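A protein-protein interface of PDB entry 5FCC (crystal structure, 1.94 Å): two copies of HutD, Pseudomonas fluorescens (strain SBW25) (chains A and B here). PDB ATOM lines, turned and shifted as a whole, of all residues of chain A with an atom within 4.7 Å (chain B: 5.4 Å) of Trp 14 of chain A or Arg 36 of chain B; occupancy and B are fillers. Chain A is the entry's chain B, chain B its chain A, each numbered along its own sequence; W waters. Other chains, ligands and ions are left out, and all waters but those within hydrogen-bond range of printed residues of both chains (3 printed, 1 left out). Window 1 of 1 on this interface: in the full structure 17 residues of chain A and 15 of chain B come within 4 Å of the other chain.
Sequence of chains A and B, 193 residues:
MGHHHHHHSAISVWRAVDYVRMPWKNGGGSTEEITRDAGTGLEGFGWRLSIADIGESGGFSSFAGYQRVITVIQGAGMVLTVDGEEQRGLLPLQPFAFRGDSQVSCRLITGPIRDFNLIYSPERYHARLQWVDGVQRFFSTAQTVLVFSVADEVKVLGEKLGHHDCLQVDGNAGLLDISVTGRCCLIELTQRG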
ATOM      1  N   SER A  12     -11.107   9.120 -26.304  1.00  0.00           N
ATOM      2  CA  SER A  12     -12.302   8.500 -25.743  1.00  0.00           C
ATOM      3  C   SER A  12     -13.417   9.525 -25.676  1.00  0.00           C
ATOM      4  O   SER A  12     -13.175  10.723 -25.513  1.00  0.00           O
ATOM      5  CB  SER A  12     -12.058   7.931 -24.342  1.00  0.00           C
ATOM      6  OG  SER A  12     -10.894   7.131 -24.296  1.00  0.00           O
ATOM      7  N   VAL A  13     -14.653   9.062 -25.819  1.00  0.00           N
ATOM      8  CA  VAL A  13     -15.791   9.954 -25.737  1.00  0.00           C
ATOM      9  C   VAL A  13     -16.692   9.453 -24.621  1.00  0.00           C
ATOM     10  O   VAL A  13     -17.089   8.278 -24.604  1.00  0.00           O
ATOM     11  CB  VAL A  13     -16.567  10.071 -27.062  1.00  0.00           C
ATOM     12  CG1 VAL A  13     -17.715  11.091 -26.897  1.00  0.00           C
ATOM     13  CG2 VAL A  13     -15.662  10.500 -28.180  1.00  0.00           C
ATOM     14  N   TRP A  14     -17.009  10.338 -23.694  1.00  0.00           N
ATOM     15  CA  TRP A  14     -17.971  10.050 -22.658  1.00  0.00           C
ATOM     16  C   TRP A  14     -19.306  10.659 -23.070  1.00  0.00           C
ATOM     17  O   TRP A  14     -19.401  11.873 -23.278  1.00  0.00           O
ATOM     18  CB  TRP A  14     -17.504  10.603 -21.319  1.00  0.00           C
ATOM     19  CG  TRP A  14     -16.082  10.222 -20.995  1.00  0.00           C
ATOM     20  CD1 TRP A  14     -14.957  10.944 -21.258  1.00  0.00           C
ATOM     21  CD2 TRP A  14     -15.653   9.035 -20.318  1.00  0.00           C
ATOM     22  NE1 TRP A  14     -13.831  10.271 -20.793  1.00  0.00           N
ATOM     23  CE2 TRP A  14     -14.239   9.092 -20.220  1.00  0.00           C
ATOM     24  CE3 TRP A  14     -16.329   7.932 -19.763  1.00  0.00           C
ATOM     25  CZ2 TRP A  14     -13.491   8.083 -19.602  1.00  0.00           C
ATOM     26  CZ3 TRP A  14     -15.578   6.931 -19.132  1.00  0.00           C
ATOM     27  CH2 TRP A  14     -14.177   7.018 -19.060  1.00  0.00           C
ATOM     28  N   ARG A  15     -20.323   9.814 -23.218  1.00  0.00           N
ATOM     29  CA  ARG A  15     -21.643  10.278 -23.599  1.00  0.00           C
ATOM     30  C   ARG A  15     -22.471  10.509 -22.348  1.00  0.00           C
ATOM     31  O   ARG A  15     -22.541   9.646 -21.450  1.00  0.00           O
ATOM     32  CB  ARG A  15     -22.329   9.269 -24.518  1.00  0.00           C
ATOM     33  CG  ARG A  15     -21.619   9.047 -25.827  1.00  0.00           C
ATOM     34  CD  ARG A  15     -21.557  10.313 -26.652  1.00  0.00           C
ATOM     35  NE  ARG A  15     -20.903  10.031 -27.921  1.00  0.00           N
ATOM     36  CZ  ARG A  15     -20.700  10.930 -28.877  1.00  0.00           C
ATOM     37  NH1 ARG A  15     -21.085  12.198 -28.695  1.00  0.00           N
ATOM     38  NH2 ARG A  15     -20.074  10.571 -29.995  1.00  0.00           N
ATOM     39  N   ALA A  16     -23.089  11.684 -22.289  1.00  0.00           N
ATOM     40  CA  ALA A  16     -23.793  12.075 -21.072  1.00  0.00           C
ATOM     41  C   ALA A  16     -24.958  11.138 -20.776  1.00  0.00           C
ATOM     42  O   ALA A  16     -25.263  10.877 -19.609  1.00  0.00           O
ATOM     43  CB  ALA A  16     -24.275  13.524 -21.185  1.00  0.00           C
ATOM     44  N   ASP A  18     -24.878   8.162 -20.858  1.00  0.00           N
ATOM     45  CA  ASP A  18     -24.302   7.070 -20.091  1.00  0.00           C
ATOM     46  C   ASP A  18     -23.863   7.464 -18.686  1.00  0.00           C
ATOM     47  O   ASP A  18     -23.377   6.604 -17.941  1.00  0.00           O
ATOM     48  CB  ASP A  18     -23.136   6.480 -20.874  1.00  0.00           C
ATOM     49  CG  ASP A  18     -23.597   5.887 -22.179  1.00  0.00           C
ATOM     50  OD1 ASP A  18     -24.746   5.411 -22.212  1.00  0.00           O
ATOM     51  OD2 ASP A  18     -22.859   5.923 -23.177  1.00  0.00           O
ATOM     52  N   TYR A  19     -24.001   8.730 -18.295  1.00  0.00           N
ATOM     53  CA  TYR A  19     -23.553   9.097 -16.961  1.00  0.00           C
ATOM     54  C   TYR A  19     -24.493   8.507 -15.932  1.00  0.00           C
ATOM     55  O   TYR A  19     -25.703   8.418 -16.153  1.00  0.00           O
ATOM     56  CB  TYR A  19     -23.510  10.620 -16.761  1.00  0.00           C
ATOM     57  CG  TYR A  19     -22.564  11.374 -17.677  1.00  0.00           C
ATOM     58  CD1 TYR A  19     -21.544  10.723 -18.354  1.00  0.00           C
ATOM     59  CD2 TYR A  19     -22.708  12.745 -17.855  1.00  0.00           C
ATOM     60  CE1 TYR A  19     -20.695  11.414 -19.196  1.00  0.00           C
ATOM     61  CE2 TYR A  19     -21.871  13.447 -18.692  1.00  0.00           C
ATOM     62  CZ  TYR A  19     -20.867  12.780 -19.359  1.00  0.00           C
ATOM     63  OH  TYR A  19     -20.047  13.488 -20.194  1.00  0.00           O
ATOM     64  N   ILE A  34     -17.960  12.074 -14.806  1.00  0.00           N
ATOM     65  CA  ILE A  34     -17.677  12.013 -16.235  1.00  0.00           C
ATOM     66  C   ILE A  34     -16.423  11.187 -16.447  1.00  0.00           C
ATOM     67  O   ILE A  34     -16.438  10.178 -17.154  1.00  0.00           O
ATOM     68  CB  ILE A  34     -17.509  13.407 -16.837  1.00  0.00           C
ATOM     69  CG1 ILE A  34     -18.806  14.186 -16.636  1.00  0.00           C
ATOM     70  CG2 ILE A  34     -17.062  13.290 -18.313  1.00  0.00           C
ATOM     71  CD1 ILE A  34     -18.665  15.663 -17.006  1.00  0.00           C
ATOM     72  N   THR A  35     -15.337  11.602 -15.815  1.00  0.00           N
ATOM     73  CA  THR A  35     -14.060  10.935 -15.980  1.00  0.00           C
ATOM     74  C   THR A  35     -13.153  11.467 -14.884  1.00  0.00           C
ATOM     75  O   THR A  35     -13.516  12.390 -14.152  1.00  0.00           O
ATOM     76  CB  THR A  35     -13.499  11.172 -17.377  1.00  0.00           C
ATOM     77  OG1 THR A  35     -12.251  10.494 -17.540  1.00  0.00           O
ATOM     78  CG2 THR A  35     -13.315  12.677 -17.652  1.00  0.00           C
ATOM     79  N   HIS A 164     -23.493  17.875 -23.078  1.00  0.00           N
ATOM     80  CA  HIS A 164     -22.736  17.371 -21.932  1.00  0.00           C
ATOM     81  C   HIS A 164     -21.919  16.136 -22.228  1.00  0.00           C
ATOM     82  O   HIS A 164     -21.357  15.569 -21.289  1.00  0.00           O
ATOM     83  CB  HIS A 164     -23.627  17.081 -20.730  1.00  0.00           C
ATOM     84  CG  HIS A 164     -24.357  18.290 -20.262  1.00  0.00           C
ATOM     85  ND1 HIS A 164     -25.291  18.258 -19.251  1.00  0.00           N
ATOM     86  CD2 HIS A 164     -24.273  19.583 -20.665  1.00  0.00           C
ATOM     87  CE1 HIS A 164     -25.777  19.475 -19.072  1.00  0.00           C
ATOM     88  NE2 HIS A 164     -25.171  20.297 -19.910  1.00  0.00           N
ATOM     89  N   ASP A 165     -21.785  15.744 -23.496  1.00  0.00           N
ATOM     90  CA  ASP A 165     -20.764  14.765 -23.865  1.00  0.00           C
ATOM     91  C   ASP A 165     -19.383  15.354 -23.644  1.00  0.00           C
ATOM     92  O   ASP A 165     -19.180  16.581 -23.662  1.00  0.00           O
ATOM     93  CB  ASP A 165     -20.892  14.344 -25.320  1.00  0.00           C
ATOM     94  CG  ASP A 165     -22.211  13.629 -25.611  1.00  0.00           C
ATOM     95  OD1 ASP A 165     -22.878  13.161 -24.660  1.00  0.00           O
ATOM     96  OD2 ASP A 165     -22.572  13.565 -26.805  1.00  0.00           O
ATOM     97  N   CYS A 166     -18.431  14.466 -23.411  1.00  0.00           N
ATOM     98  CA  CYS A 166     -17.070  14.859 -23.102  1.00  0.00           C
ATOM     99  C   CYS A 166     -16.098  14.014 -23.905  1.00  0.00           C
ATOM    100  O   CYS A 166     -16.078  12.783 -23.781  1.00  0.00           O
ATOM    101  CB  CYS A 166     -16.786  14.723 -21.612  1.00  0.00           C
ATOM    102  SG  CYS A 166     -15.142  15.360 -21.172  1.00  0.00           S
ATOM    103  N   GLN A 168     -12.219  12.974 -24.484  1.00  0.00           N
ATOM    104  CA  GLN A 168     -10.972  12.922 -23.720  1.00  0.00           C
ATOM    105  C   GLN A 168      -9.857  12.367 -24.588  1.00  0.00           C
ATOM    106  O   GLN A 168      -9.952  11.234 -25.080  1.00  0.00           O
ATOM    107  CB  GLN A 168     -11.124  12.051 -22.465  1.00  0.00           C
ATOM    108  CG  GLN A 168      -9.854  11.837 -21.664  1.00  0.00           C
ATOM    109  CD  GLN A 168     -10.130  11.201 -20.286  1.00  0.00           C
ATOM    110  OE1 GLN A 168     -11.282  11.068 -19.862  1.00  0.00           O
ATOM    111  NE2 GLN A 168      -9.061  10.818 -19.580  1.00  0.00           N
ATOM    112  N   MET B  22     -14.483   3.385 -11.110  1.00  0.00           N
ATOM    113  CA  MET B  22     -15.633   4.103 -10.572  1.00  0.00           C
ATOM    114  C   MET B  22     -16.397   3.186  -9.644  1.00  0.00           C
ATOM    115  O   MET B  22     -16.758   2.063 -10.036  1.00  0.00           O
ATOM    116  CB  MET B  22     -16.558   4.594 -11.692  1.00  0.00           C
ATOM    117  CG  MET B  22     -15.870   5.420 -12.775  1.00  0.00           C
ATOM    118  SD  MET B  22     -15.659   7.154 -12.336  1.00  0.00           S
ATOM    119  CE  MET B  22     -15.742   7.944 -13.957  1.00  0.00           C
ATOM    120  N   GLU B  33     -13.043   1.090 -16.147  1.00  0.00           N
ATOM    121  CA  GLU B  33     -13.227   1.329 -17.568  1.00  0.00           C
ATOM    122  C   GLU B  33     -11.984   0.884 -18.300  1.00  0.00           C
ATOM    123  O   GLU B  33     -10.866   1.178 -17.868  1.00  0.00           O
ATOM    124  CB  GLU B  33     -13.485   2.816 -17.827  1.00  0.00           C
ATOM    125  CG  GLU B  33     -13.486   3.176 -19.291  1.00  0.00           C
ATOM    126  CD  GLU B  33     -14.831   2.868 -19.934  1.00  0.00           C
ATOM    127  OE1 GLU B  33     -15.777   2.465 -19.195  1.00  0.00           O
ATOM    128  OE2 GLU B  33     -14.929   3.054 -21.158  1.00  0.00           O
ATOM    129  N   ILE B  34     -12.170   0.131 -19.381  1.00  0.00           N
ATOM    130  CA  ILE B  34     -11.052  -0.206 -20.243  1.00  0.00           C
ATOM    131  C   ILE B  34     -11.140   0.693 -21.462  1.00  0.00           C
ATOM    132  O   ILE B  34     -10.217   1.458 -21.761  1.00  0.00           O
ATOM    133  CB  ILE B  34     -11.063  -1.687 -20.656  1.00  0.00           C
ATOM    134  CG1 ILE B  34     -10.933  -2.605 -19.435  1.00  0.00           C
ATOM    135  CG2 ILE B  34      -9.986  -1.931 -21.674  1.00  0.00           C
ATOM    136  CD1 ILE B  34     -10.876  -4.136 -19.811  1.00  0.00           C
ATOM    137  N   THR B  35     -12.234   0.570 -22.203  1.00  0.00           N
ATOM    138  CA  THR B  35     -12.394   1.357 -23.418  1.00  0.00           C
ATOM    139  C   THR B  35     -13.830   1.158 -23.893  1.00  0.00           C
ATOM    140  O   THR B  35     -14.477   0.166 -23.546  1.00  0.00           O
ATOM    141  CB  THR B  35     -11.368   0.950 -24.492  1.00  0.00           C
ATOM    142  OG1 THR B  35     -11.531   1.733 -25.675  1.00  0.00           O
ATOM    143  CG2 THR B  35     -11.553  -0.516 -24.888  1.00  0.00           C
ATOM    144  N   ARG B  36     -14.339   2.119 -24.650  1.00  0.00           N
ATOM    145  CA  ARG B  36     -15.699   2.018 -25.144  1.00  0.00           C
ATOM    146  C   ARG B  36     -15.721   2.674 -26.507  1.00  0.00           C
ATOM    147  O   ARG B  36     -14.769   3.352 -26.884  1.00  0.00           O
ATOM    148  CB  ARG B  36     -16.695   2.658 -24.185  1.00  0.00           C
ATOM    149  CG  ARG B  36     -16.517   4.172 -24.027  1.00  0.00           C
ATOM    150  CD  ARG B  36     -17.564   4.760 -23.147  1.00  0.00           C
ATOM    151  NE  ARG B  36     -17.393   4.293 -21.789  1.00  0.00           N
ATOM    152  CZ  ARG B  36     -18.119   4.711 -20.772  1.00  0.00           C
ATOM    153  NH1 ARG B  36     -19.081   5.609 -20.968  1.00  0.00           N
ATOM    154  NH2 ARG B  36     -17.885   4.233 -19.571  1.00  0.00           N
ATOM    155  N   ASP B  37     -16.757   2.411 -27.299  1.00  0.00           N
ATOM    156  CA  ASP B  37     -16.702   3.118 -28.563  1.00  0.00           C
ATOM    157  C   ASP B  37     -17.138   4.576 -28.367  1.00  0.00           C
ATOM    158  O   ASP B  37     -17.696   4.957 -27.337  1.00  0.00           O
ATOM    159  CB  ASP B  37     -17.566   2.456 -29.617  1.00  0.00           C
ATOM    160  CG  ASP B  37     -19.000   2.735 -29.406  1.00  0.00           C
ATOM    161  OD1 ASP B  37     -19.391   2.695 -28.237  1.00  0.00           O
ATOM    162  OD2 ASP B  37     -19.724   2.976 -30.374  1.00  0.00           O
ATOM    163  N   ALA B  38     -16.936   5.372 -29.408  1.00  0.00           N
ATOM    164  CA  ALA B  38     -17.254   6.782 -29.296  1.00  0.00           C
ATOM    165  C   ALA B  38     -18.743   6.987 -29.047  1.00  0.00           C
ATOM    166  O   ALA B  38     -19.146   7.988 -28.448  1.00  0.00           O
ATOM    167  CB  ALA B  38     -16.795   7.499 -30.562  1.00  0.00           C
ATOM    168  N   PHE B  45     -22.703   4.895 -25.684  1.00  0.00           N
ATOM    169  CA  PHE B  45     -21.778   3.937 -26.272  1.00  0.00           C
ATOM    170  C   PHE B  45     -22.538   2.769 -26.902  1.00  0.00           C
ATOM    171  O   PHE B  45     -23.599   2.366 -26.426  1.00  0.00           O
ATOM    172  CB  PHE B  45     -20.764   3.437 -25.244  1.00  0.00           C
ATOM    173  CG  PHE B  45     -21.337   2.666 -24.084  1.00  0.00           C
ATOM    174  CD1 PHE B  45     -21.709   1.315 -24.220  1.00  0.00           C
ATOM    175  CD2 PHE B  45     -21.385   3.240 -22.815  1.00  0.00           C
ATOM    176  CE1 PHE B  45     -22.194   0.599 -23.144  1.00  0.00           C
ATOM    177  CE2 PHE B  45     -21.854   2.511 -21.712  1.00  0.00           C
ATOM    178  CZ  PHE B  45     -22.264   1.181 -21.881  1.00  0.00           C
ATOM    179  N   TRP B  47     -20.682  -0.056 -27.578  1.00  0.00           N
ATOM    180  CA  TRP B  47     -20.073  -1.167 -26.875  1.00  0.00           C
ATOM    181  C   TRP B  47     -19.121  -0.616 -25.830  1.00  0.00           C
ATOM    182  O   TRP B  47     -18.674   0.538 -25.913  1.00  0.00           O
ATOM    183  CB  TRP B  47     -19.335  -2.099 -27.832  1.00  0.00           C
ATOM    184  CG  TRP B  47     -18.283  -1.460 -28.679  1.00  0.00           C
ATOM    185  CD1 TRP B  47     -18.394  -1.061 -29.990  1.00  0.00           C
ATOM    186  CD2 TRP B  47     -16.936  -1.176 -28.287  1.00  0.00           C
ATOM    187  NE1 TRP B  47     -17.181  -0.564 -30.445  1.00  0.00           N
ATOM    188  CE2 TRP B  47     -16.276  -0.616 -29.412  1.00  0.00           C
ATOM    189  CE3 TRP B  47     -16.217  -1.369 -27.115  1.00  0.00           C
ATOM    190  CZ2 TRP B  47     -14.951  -0.207 -29.364  1.00  0.00           C
ATOM    191  CZ3 TRP B  47     -14.899  -0.967 -27.072  1.00  0.00           C
ATOM    192  CH2 TRP B  47     -14.272  -0.411 -28.186  1.00  0.00           C
ATOM    193  N   ARG B  48     -18.771  -1.480 -24.880  1.00  0.00           N
ATOM    194  CA  ARG B  48     -17.880  -1.115 -23.790  1.00  0.00           C
ATOM    195  C   ARG B  48     -17.154  -2.357 -23.271  1.00  0.00           C
ATOM    196  O   ARG B  48     -17.739  -3.432 -23.178  1.00  0.00           O
ATOM    197  CB  ARG B  48     -18.685  -0.439 -22.676  1.00  0.00           C
ATOM    198  CG  ARG B  48     -17.846   0.019 -21.519  1.00  0.00           C
ATOM    199  CD  ARG B  48     -18.737   0.375 -20.361  1.00  0.00           C
ATOM    200  NE  ARG B  48     -17.919   0.932 -19.295  1.00  0.00           N
ATOM    201  CZ  ARG B  48     -18.354   1.093 -18.055  1.00  0.00           C
ATOM    202  NH1 ARG B  48     -19.596   0.725 -17.753  1.00  0.00           N
ATOM    203  NH2 ARG B  48     -17.544   1.621 -17.135  1.00  0.00           N
ATOM    204  N   LEU B  49     -15.866  -2.205 -22.983  1.00  0.00           N
ATOM    205  CA  LEU B  49     -15.098  -3.184 -22.235  1.00  0.00           C
ATOM    206  C   LEU B  49     -14.813  -2.612 -20.863  1.00  0.00           C
ATOM    207  O   LEU B  49     -14.462  -1.430 -20.735  1.00  0.00           O
ATOM    208  CB  LEU B  49     -13.784  -3.506 -22.911  1.00  0.00           C
ATOM    209  CG  LEU B  49     -13.743  -4.669 -23.865  1.00  0.00           C
ATOM    210  CD1 LEU B  49     -14.885  -4.603 -24.772  1.00  0.00           C
ATOM    211  CD2 LEU B  49     -12.479  -4.559 -24.622  1.00  0.00           C
ATOM    212  N   GLN B 168      -6.288  -2.456 -28.659  1.00  0.00           N
ATOM    213  CA  GLN B 168      -7.452  -2.073 -29.449  1.00  0.00           C
ATOM    214  C   GLN B 168      -6.978  -1.642 -30.826  1.00  0.00           C
ATOM    215  O   GLN B 168      -6.070  -0.811 -30.938  1.00  0.00           O
ATOM    216  CB  GLN B 168      -8.244  -0.941 -28.781  1.00  0.00           C
ATOM    217  CG  GLN B 168      -9.411  -0.366 -29.637  1.00  0.00           C
ATOM    218  CD  GLN B 168     -10.287   0.568 -28.830  1.00  0.00           C
ATOM    219  OE1 GLN B 168     -10.134   0.672 -27.609  1.00  0.00           O
ATOM    220  NE2 GLN B 168     -11.252   1.219 -29.490  1.00  0.00           N
HETATM  221  O   HOH W   1     -25.095   3.257 -23.861  1.00  0.00           O
HETATM  222  O   HOH W   2     -20.321   6.921 -23.084  1.00  0.00           O
HETATM  223  O   HOH W   3     -14.726   6.295 -26.613  1.00  0.00           O
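O of Ala 38 of chain B is in hydrogen-bond range of NE of Arg 15 of chain A, at 2.7 Å.
N of Phe 45 of chain B sits at hydrogen-bond distance from OD2 of Asp 18 of chain A (2.7 Å).
The backbone NH (N) of Trp 14 of chain A lies within hydrogen-bond range of the backbone carbonyl oxygen (O) of Cys 166 of chain A (2.6 Å).
OG1 of Thr 35 of chain A lies within hydrogen-bond range of OE1 of Gln 168 of chain A (2.6 Å).
The guanidinium group of Arg 15 of chain A is in salt-bridge range of the side-chain carboxylate of Asp 165 of chain A (2.8 Å).
NE1 of Trp 14 of chain A sits at hydrogen-bond distance from OE1 of Gln 168 of chain A (2.8 Å).
The guanidinium group (NH2) of Arg 36 of chain B is in salt-bridge range of the side-chain carboxylate (OE1) of Glu 33 of chain B (2.8 Å).
The guanidinium group (NE) of Arg 48 of chain B is in salt-bridge range of the side-chain carboxylate (OE1) of Glu 33 of chain B (2.6 Å).
Among the printed residues, merely in contact across the chains: Trp 14 of chain A with Arg 36 of chain B (3.6 Å), Val 13 of chain A with Ala 38 of chain B (3.6 Å), Val 13 of chain A with Arg 36 of chain B (3.8 Å), Trp 14 of chain A with Glu 33 of chain B (3.9 Å), Ile 34 of chain A with Met 22 of chain B (3.96 Å) and Thr 35 of chain A with Met 22 of chain B (3.98 Å).
Of the printed residues of chain B, Trp 14 of chain A touches Glu 33 and Arg 36.
Of the printed residues of chain B, Asp 18 of chain A touches Phe 45 (2.7 Å).
Cys 166 of chain A touches none of the printed residues of chain B.
Arg 36 of chain B touches just these residues of chain A: Val 13 (3.8 Å) and Trp 14 (3.6 Å).
Asp 37 of chain B touches none of the printed residues of chain A.
Of the printed residues of chain A, Ala 38 of chain B touches Val 13 (3.6 Å) and Arg 15 (2.7 Å).
Printed residues of chain A within 4 Å of Phe 45 of chain B: Asp 18 (2.7 Å).
Hydrophobic or aromatic side chains of chain B within 4 Å of the printed part of chain A: Met 22, Ala 38 and Phe 45.
Among the printed residues, 8 pairs touch across the chains.
Positions printed for both chains: 34, 35 and 168.
Of the 8 pairs that touch across the chains among the printed residues, none has its exchanged pair printed and touching as well.
Water W2 lies within hydrogen-bond range of OD2 of Asp 18 of chain A (2.7 Å), NH1 of Arg 36 of chain B (2.8 Å) and N of Arg 15 of chain A (2.9 Å).
Water W1 lies within hydrogen-bond range of the side-chain carboxylate (OD1) of Asp 18 of chain A (2.7 Å) and the backbone carbonyl oxygen (O) of Phe 45 of chain B (3.1 Å).
Water W3 lies within hydrogen-bond range of the backbone NH of Val 13 of chain A (2.9 Å), the backbone carbonyl oxygen of Arg 36 of chain B (3.0 Å) and the backbone carbonyl oxygen of Asp 37 of chain B (3.3 Å).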
